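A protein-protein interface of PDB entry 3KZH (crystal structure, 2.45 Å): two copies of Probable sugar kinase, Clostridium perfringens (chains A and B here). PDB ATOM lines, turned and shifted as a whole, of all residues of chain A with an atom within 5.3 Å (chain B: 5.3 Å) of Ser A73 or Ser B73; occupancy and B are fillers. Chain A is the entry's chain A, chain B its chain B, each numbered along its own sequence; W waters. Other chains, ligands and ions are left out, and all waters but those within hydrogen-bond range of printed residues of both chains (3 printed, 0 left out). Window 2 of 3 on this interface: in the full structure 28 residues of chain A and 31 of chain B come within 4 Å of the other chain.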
ATOM      1  N   PHE A  41      10.670  -5.157 -14.771  1.00  0.00           N
ATOM      2  CA  PHE A  41      10.574  -5.969 -15.978  1.00  0.00           C
ATOM      3  C   PHE A  41      10.308  -5.101 -17.202  1.00  0.00           C
ATOM      4  O   PHE A  41       9.424  -4.239 -17.192  1.00  0.00           O
ATOM      5  CB  PHE A  41       9.478  -7.022 -15.829  1.00  0.00           C
ATOM      6  CG  PHE A  41       9.665  -7.945 -14.659  1.00  0.00           C
ATOM      7  CD1 PHE A  41      10.894  -8.598 -14.435  1.00  0.00           C
ATOM      8  CD2 PHE A  41       8.593  -8.201 -13.791  1.00  0.00           C
ATOM      9  CE1 PHE A  41      11.058  -9.498 -13.362  1.00  0.00           C
ATOM     10  CE2 PHE A  41       8.745  -9.100 -12.708  1.00  0.00           C
ATOM     11  CZ  PHE A  41       9.978  -9.752 -12.500  1.00  0.00           C
ATOM     12  N   GLU A  69      17.857 -17.156 -12.249  1.00  0.00           N
ATOM     13  CA  GLU A  69      16.959 -16.549 -11.264  1.00  0.00           C
ATOM     14  C   GLU A  69      16.022 -15.477 -11.824  1.00  0.00           C
ATOM     15  O   GLU A  69      14.903 -15.312 -11.336  1.00  0.00           O
ATOM     16  CB  GLU A  69      17.766 -15.989 -10.091  1.00  0.00           C
ATOM     17  CG  GLU A  69      17.177 -16.313  -8.721  1.00  0.00           C
ATOM     18  CD  GLU A  69      17.294 -17.788  -8.331  1.00  0.00           C
ATOM     19  OE1 GLU A  69      16.329 -18.322  -7.747  1.00  0.00           O
ATOM     20  OE2 GLU A  69      18.347 -18.412  -8.581  1.00  0.00           O
ATOM     21  N   HIS A  70      16.482 -14.761 -12.847  1.00  0.00           N
ATOM     22  CA  HIS A  70      15.681 -13.725 -13.495  1.00  0.00           C
ATOM     23  C   HIS A  70      14.630 -14.366 -14.385  1.00  0.00           C
ATOM     24  O   HIS A  70      13.573 -13.780 -14.625  1.00  0.00           O
ATOM     25  CB  HIS A  70      16.552 -12.781 -14.314  1.00  0.00           C
ATOM     26  CG  HIS A  70      17.275 -11.759 -13.493  1.00  0.00           C
ATOM     27  ND1 HIS A  70      16.880 -11.403 -12.222  1.00  0.00           N
ATOM     28  CD2 HIS A  70      18.366 -11.014 -13.772  1.00  0.00           C
ATOM     29  CE1 HIS A  70      17.698 -10.478 -11.754  1.00  0.00           C
ATOM     30  NE2 HIS A  70      18.608 -10.223 -12.674  1.00  0.00           N
ATOM     31  N   GLY A  71      14.925 -15.590 -14.829  1.00  0.00           N
ATOM     32  CA  GLY A  71      14.013 -16.366 -15.654  1.00  0.00           C
ATOM     33  C   GLY A  71      12.828 -16.800 -14.819  1.00  0.00           C
ATOM     34  O   GLY A  71      11.695 -16.697 -15.272  1.00  0.00           O
ATOM     35  N   LYS A  72      13.092 -17.189 -13.569  1.00  0.00           N
ATOM     36  CA  LYS A  72      12.044 -17.613 -12.631  1.00  0.00           C
ATOM     37  C   LYS A  72      11.182 -16.428 -12.186  1.00  0.00           C
ATOM     38  O   LYS A  72       9.994 -16.598 -11.894  1.00  0.00           O
ATOM     39  CB  LYS A  72      12.652 -18.288 -11.394  1.00  0.00           C
ATOM     40  CG  LYS A  72      13.578 -19.434 -11.712  1.00  0.00           C
ATOM     41  CD  LYS A  72      14.104 -20.110 -10.454  1.00  0.00           C
ATOM     42  CE  LYS A  72      15.438 -20.791 -10.724  1.00  0.00           C
ATOM     43  NZ  LYS A  72      15.430 -21.640 -11.952  1.00  0.00           N
ATOM     44  N   SER A  73      11.787 -15.237 -12.173  1.00  0.00           N
ATOM     45  CA  SER A  73      11.120 -13.987 -11.786  1.00  0.00           C
ATOM     46  C   SER A  73      10.054 -13.597 -12.815  1.00  0.00           C
ATOM     47  O   SER A  73       8.919 -13.271 -12.451  1.00  0.00           O
ATOM     48  CB  SER A  73      12.139 -12.853 -11.657  1.00  0.00           C
ATOM     49  OG  SER A  73      13.088 -13.110 -10.650  1.00  0.00           O
ATOM     50  N   ILE A  74      10.433 -13.668 -14.095  1.00  0.00           N
ATOM     51  CA  ILE A  74       9.551 -13.364 -15.232  1.00  0.00           C
ATOM     52  C   ILE A  74       8.389 -14.366 -15.240  1.00  0.00           C
ATOM     53  O   ILE A  74       7.230 -13.951 -15.239  1.00  0.00           O
ATOM     54  CB  ILE A  74      10.314 -13.450 -16.600  1.00  0.00           C
ATOM     55  CG1 ILE A  74      11.468 -12.446 -16.659  1.00  0.00           C
ATOM     56  CG2 ILE A  74       9.360 -13.223 -17.786  1.00  0.00           C
ATOM     57  CD1 ILE A  74      11.094 -11.015 -17.058  1.00  0.00           C
ATOM     58  N   VAL A  75       8.707 -15.664 -15.158  1.00  0.00           N
ATOM     59  CA  VAL A  75       7.707 -16.732 -15.165  1.00  0.00           C
ATOM     60  C   VAL A  75       6.690 -16.578 -14.047  1.00  0.00           C
ATOM     61  O   VAL A  75       5.487 -16.661 -14.300  1.00  0.00           O
ATOM     62  CB  VAL A  75       8.347 -18.155 -15.138  1.00  0.00           C
ATOM     63  CG1 VAL A  75       7.267 -19.237 -15.235  1.00  0.00           C
ATOM     64  CG2 VAL A  75       9.259 -18.335 -16.290  1.00  0.00           C
ATOM     65  N   GLU A  76       7.169 -16.277 -12.838  1.00  0.00           N
ATOM     66  CA  GLU A  76       6.280 -16.074 -11.691  1.00  0.00           C
ATOM     67  C   GLU A  76       5.362 -14.869 -11.866  1.00  0.00           C
ATOM     68  O   GLU A  76       4.181 -14.939 -11.526  1.00  0.00           O
ATOM     69  CB  GLU A  76       7.065 -15.958 -10.372  1.00  0.00           C
ATOM     70  CG  GLU A  76       7.457 -17.305  -9.741  1.00  0.00           C
ATOM     71  CD  GLU A  76       6.267 -18.254  -9.537  1.00  0.00           C
ATOM     72  OE1 GLU A  76       5.284 -17.868  -8.857  1.00  0.00           O
ATOM     73  OE2 GLU A  76       6.313 -19.380 -10.077  1.00  0.00           O
ATOM     74  N   HIS A  77       5.885 -13.799 -12.474  1.00  0.00           N
ATOM     75  CA  HIS A  77       5.093 -12.592 -12.728  1.00  0.00           C
ATOM     76  C   HIS A  77       4.034 -12.874 -13.801  1.00  0.00           C
ATOM     77  O   HIS A  77       2.913 -12.390 -13.702  1.00  0.00           O
ATOM     78  CB  HIS A  77       6.000 -11.433 -13.144  1.00  0.00           C
ATOM     79  CG  HIS A  77       5.284 -10.126 -13.308  1.00  0.00           C
ATOM     80  ND1 HIS A  77       4.804  -9.401 -12.238  1.00  0.00           N
ATOM     81  CD2 HIS A  77       4.983  -9.406 -14.412  1.00  0.00           C
ATOM     82  CE1 HIS A  77       4.240  -8.290 -12.680  1.00  0.00           C
ATOM     83  NE2 HIS A  77       4.337  -8.271 -13.994  1.00  0.00           N
ATOM     84  N   SER A  78       4.388 -13.731 -14.763  1.00  0.00           N
ATOM     85  CA  SER A  78       3.486 -14.129 -15.840  1.00  0.00           C
ATOM     86  C   SER A  78       2.312 -14.971 -15.362  1.00  0.00           C
ATOM     87  O   SER A  78       1.213 -14.857 -15.899  1.00  0.00           O
ATOM     88  CB  SER A  78       4.257 -14.825 -16.971  1.00  0.00           C
ATOM     89  OG  SER A  78       4.727 -16.115 -16.638  1.00  0.00           O
ATOM     90  N   PHE B  41      22.687 -15.516  -3.628  1.00  0.00           N
ATOM     91  CA  PHE B  41      22.094 -15.181  -2.340  1.00  0.00           C
ATOM     92  C   PHE B  41      23.115 -15.315  -1.216  1.00  0.00           C
ATOM     93  O   PHE B  41      23.598 -16.414  -0.937  1.00  0.00           O
ATOM     94  CB  PHE B  41      20.861 -16.047  -2.088  1.00  0.00           C
ATOM     95  CG  PHE B  41      19.816 -15.952  -3.167  1.00  0.00           C
ATOM     96  CD1 PHE B  41      19.265 -14.704  -3.537  1.00  0.00           C
ATOM     97  CD2 PHE B  41      19.350 -17.115  -3.805  1.00  0.00           C
ATOM     98  CE1 PHE B  41      18.263 -14.613  -4.533  1.00  0.00           C
ATOM     99  CE2 PHE B  41      18.347 -17.039  -4.806  1.00  0.00           C
ATOM    100  CZ  PHE B  41      17.803 -15.785  -5.161  1.00  0.00           C
ATOM    101  N   GLU B  69      11.284  -7.867  -6.162  1.00  0.00           N
ATOM    102  CA  GLU B  69      11.606  -9.106  -6.872  1.00  0.00           C
ATOM    103  C   GLU B  69      12.696  -9.959  -6.245  1.00  0.00           C
ATOM    104  O   GLU B  69      12.601 -11.186  -6.252  1.00  0.00           O
ATOM    105  CB  GLU B  69      11.928  -8.818  -8.341  1.00  0.00           C
ATOM    106  CG  GLU B  69      10.766  -8.216  -9.124  1.00  0.00           C
ATOM    107  CD  GLU B  69       9.497  -9.065  -9.076  1.00  0.00           C
ATOM    108  OE1 GLU B  69       9.581 -10.304  -9.247  1.00  0.00           O
ATOM    109  OE2 GLU B  69       8.407  -8.484  -8.880  1.00  0.00           O
ATOM    110  N   HIS B  70      13.699  -9.296  -5.670  1.00  0.00           N
ATOM    111  CA  HIS B  70      14.813  -9.958  -4.994  1.00  0.00           C
ATOM    112  C   HIS B  70      14.312 -10.654  -3.727  1.00  0.00           C
ATOM    113  O   HIS B  70      14.779 -11.737  -3.391  1.00  0.00           O
ATOM    114  CB  HIS B  70      15.910  -8.947  -4.641  1.00  0.00           C
ATOM    115  CG  HIS B  70      16.826  -8.604  -5.778  1.00  0.00           C
ATOM    116  ND1 HIS B  70      16.814  -9.277  -6.983  1.00  0.00           N
ATOM    117  CD2 HIS B  70      17.792  -7.663  -5.884  1.00  0.00           C
ATOM    118  CE1 HIS B  70      17.734  -8.764  -7.779  1.00  0.00           C
ATOM    119  NE2 HIS B  70      18.342  -7.782  -7.140  1.00  0.00           N
ATOM    120  N   GLY B  71      13.320 -10.041  -3.074  1.00  0.00           N
ATOM    121  CA  GLY B  71      12.715 -10.599  -1.872  1.00  0.00           C
ATOM    122  C   GLY B  71      11.900 -11.843  -2.165  1.00  0.00           C
ATOM    123  O   GLY B  71      11.966 -12.813  -1.417  1.00  0.00           O
ATOM    124  N   LYS B  72      11.183 -11.824  -3.292  1.00  0.00           N
ATOM    125  CA  LYS B  72      10.365 -12.954  -3.744  1.00  0.00           C
ATOM    126  C   LYS B  72      11.254 -14.129  -4.151  1.00  0.00           C
ATOM    127  O   LYS B  72      10.948 -15.266  -3.810  1.00  0.00           O
ATOM    128  CB  LYS B  72       9.469 -12.545  -4.915  1.00  0.00           C
ATOM    129  CG  LYS B  72       8.380 -11.547  -4.565  1.00  0.00           C
ATOM    130  CD  LYS B  72       7.746 -10.981  -5.822  1.00  0.00           C
ATOM    131  CE  LYS B  72       6.735  -9.900  -5.493  1.00  0.00           C
ATOM    132  NZ  LYS B  72       6.359  -9.141  -6.718  1.00  0.00           N
ATOM    133  N   SER B  73      12.385 -13.831  -4.806  1.00  0.00           N
ATOM    134  CA  SER B  73      13.365 -14.841  -5.249  1.00  0.00           C
ATOM    135  C   SER B  73      14.023 -15.556  -4.068  1.00  0.00           C
ATOM    136  O   SER B  73      14.327 -16.747  -4.150  1.00  0.00           O
ATOM    137  CB  SER B  73      14.450 -14.206  -6.121  1.00  0.00           C
ATOM    138  OG  SER B  73      13.927 -13.744  -7.352  1.00  0.00           O
ATOM    139  N   ILE B  74      14.216 -14.818  -2.972  1.00  0.00           N
ATOM    140  CA  ILE B  74      14.793 -15.339  -1.729  1.00  0.00           C
ATOM    141  C   ILE B  74      13.782 -16.314  -1.103  1.00  0.00           C
ATOM    142  O   ILE B  74      14.151 -17.429  -0.747  1.00  0.00           O
ATOM    143  CB  ILE B  74      15.159 -14.165  -0.742  1.00  0.00           C
ATOM    144  CG1 ILE B  74      16.532 -13.571  -1.089  1.00  0.00           C
ATOM    145  CG2 ILE B  74      15.105 -14.606   0.731  1.00  0.00           C
ATOM    146  CD1 ILE B  74      17.741 -14.241  -0.393  1.00  0.00           C
ATOM    147  N   VAL B  75      12.512 -15.896  -1.042  1.00  0.00           N
ATOM    148  CA  VAL B  75      11.417 -16.704  -0.488  1.00  0.00           C
ATOM    149  C   VAL B  75      11.161 -17.984  -1.305  1.00  0.00           C
ATOM    150  O   VAL B  75      10.795 -19.006  -0.732  1.00  0.00           O
ATOM    151  CB  VAL B  75      10.099 -15.878  -0.348  1.00  0.00           C
ATOM    152  CG1 VAL B  75       9.011 -16.669   0.398  1.00  0.00           C
ATOM    153  CG2 VAL B  75      10.367 -14.608   0.415  1.00  0.00           C
ATOM    154  N   GLU B  76      11.403 -17.936  -2.619  1.00  0.00           N
ATOM    155  CA  GLU B  76      11.215 -19.106  -3.484  1.00  0.00           C
ATOM    156  C   GLU B  76      12.346 -20.117  -3.323  1.00  0.00           C
ATOM    157  O   GLU B  76      12.092 -21.324  -3.322  1.00  0.00           O
ATOM    158  CB  GLU B  76      11.054 -18.716  -4.964  1.00  0.00           C
ATOM    159  CG  GLU B  76       9.832 -17.838  -5.320  1.00  0.00           C
ATOM    160  CD  GLU B  76       8.496 -18.380  -4.814  1.00  0.00           C
ATOM    161  OE1 GLU B  76       8.025 -19.414  -5.344  1.00  0.00           O
ATOM    162  OE2 GLU B  76       7.917 -17.761  -3.887  1.00  0.00           O
ATOM    163  N   HIS B  77      13.577 -19.617  -3.156  1.00  0.00           N
ATOM    164  CA  HIS B  77      14.782 -20.444  -2.949  1.00  0.00           C
ATOM    165  C   HIS B  77      14.700 -21.078  -1.552  1.00  0.00           C
ATOM    166  O   HIS B  77      15.253 -22.148  -1.312  1.00  0.00           O
ATOM    167  CB  HIS B  77      16.042 -19.568  -3.070  1.00  0.00           C
ATOM    168  CG  HIS B  77      17.342 -20.316  -2.941  1.00  0.00           C
ATOM    169  ND1 HIS B  77      17.945 -20.951  -4.009  1.00  0.00           N
ATOM    170  CD2 HIS B  77      18.166 -20.496  -1.885  1.00  0.00           C
ATOM    171  CE1 HIS B  77      19.084 -21.486  -3.609  1.00  0.00           C
ATOM    172  NE2 HIS B  77      19.245 -21.227  -2.328  1.00  0.00           N
ATOM    173  N   SER B  78      13.993 -20.391  -0.656  1.00  0.00           N
ATOM    174  CA  SER B  78      13.771 -20.813   0.725  1.00  0.00           C
ATOM    175  C   SER B  78      12.898 -22.070   0.846  1.00  0.00           C
ATOM    176  O   SER B  78      13.157 -22.930   1.694  1.00  0.00           O
ATOM    177  CB  SER B  78      13.189 -19.632   1.516  1.00  0.00           C
ATOM    178  OG  SER B  78      12.320 -20.005   2.569  1.00  0.00           O
HETATM  179  O   HOH W   1      14.010 -18.158  -6.383  1.00  0.00           O
HETATM  180  O   HOH W   2       7.898 -12.440  -9.867  1.00  0.00           O
HETATM  181  O   HOH W   3      11.529 -12.556  -8.302  1.00  0.00           O
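The side-chain hydroxyl (OG) of Ser A73 is in hydrogen-bond range of the side-chain hydroxyl (OG) of Ser B73 (3.5 Å).
O of Glu A69 sits at hydrogen-bond distance from OG of Ser A73 (2.9 Å).
The side-chain amino group of Lys B72 lies within salt-bridge range of the side-chain carboxylate of Glu B69, at 3.0 Å.
O of Glu B69 is in hydrogen-bond range of OG of Ser B73 (3.1 Å).
Among the printed residues, merely in contact across the chains: Phe A41 with Glu B69 (3.3 Å) and Glu A69 with Phe B41 (3.7 Å).
Printed residues of chain B within 4 Å of Glu A69: Phe B41.
Ser A73 touches just one residue of chain B: Ser B73.
Of the printed residues of chain A, Phe B41 touches Glu A69.
Ser B73 touches one residue of chain A.
The nearest residue of chain B that does not touch Ser A73 is Glu B69 (4.3 Å).
Hydrophobic or aromatic side chains of chain A within 4 Å of the printed part of chain B: Phe A41.
Along chain A the printed residues that touch a printed residue of chain B span positions 41 to 73.
Hydrophobic or aromatic side chains of chain B within 4 Å of the printed part of chain A: Phe B41.
Among the printed residues, 3 pairs touch across the chains.
Among the printed residues, no Asp or Glu carboxylate lies within 4 Å of a Lys or Arg side-chain nitrogen of the other chain.
Phe A41 touches Glu B69, and with the chains exchanged Glu A69 touches Phe B41.
Ser B73 touches its own counterpart, Ser A73.
Positions printed for both chains: 41, 69, 70, 71, 72, 73, 74, 75, 76, 77 and 78.
Of the 3 pairs that touch across the chains among the printed residues, 3 have their exchanged pair printed and touching as well.
Water W1 bridges O of Ser B73 (2.7 Å) and OE1 of Glu A69 (2.7 Å).
Water W3 lies within hydrogen-bond range of the backbone carbonyl oxygen of Glu B69, the side-chain hydroxyl of Ser B73 and the side-chain hydroxyl of Ser A73.
Water W2 lies within hydrogen-bond range of the side-chain carboxylate of Glu B69 (2.8 Å) and the backbone carbonyl oxygen of Ser A73 (2.9 Å).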
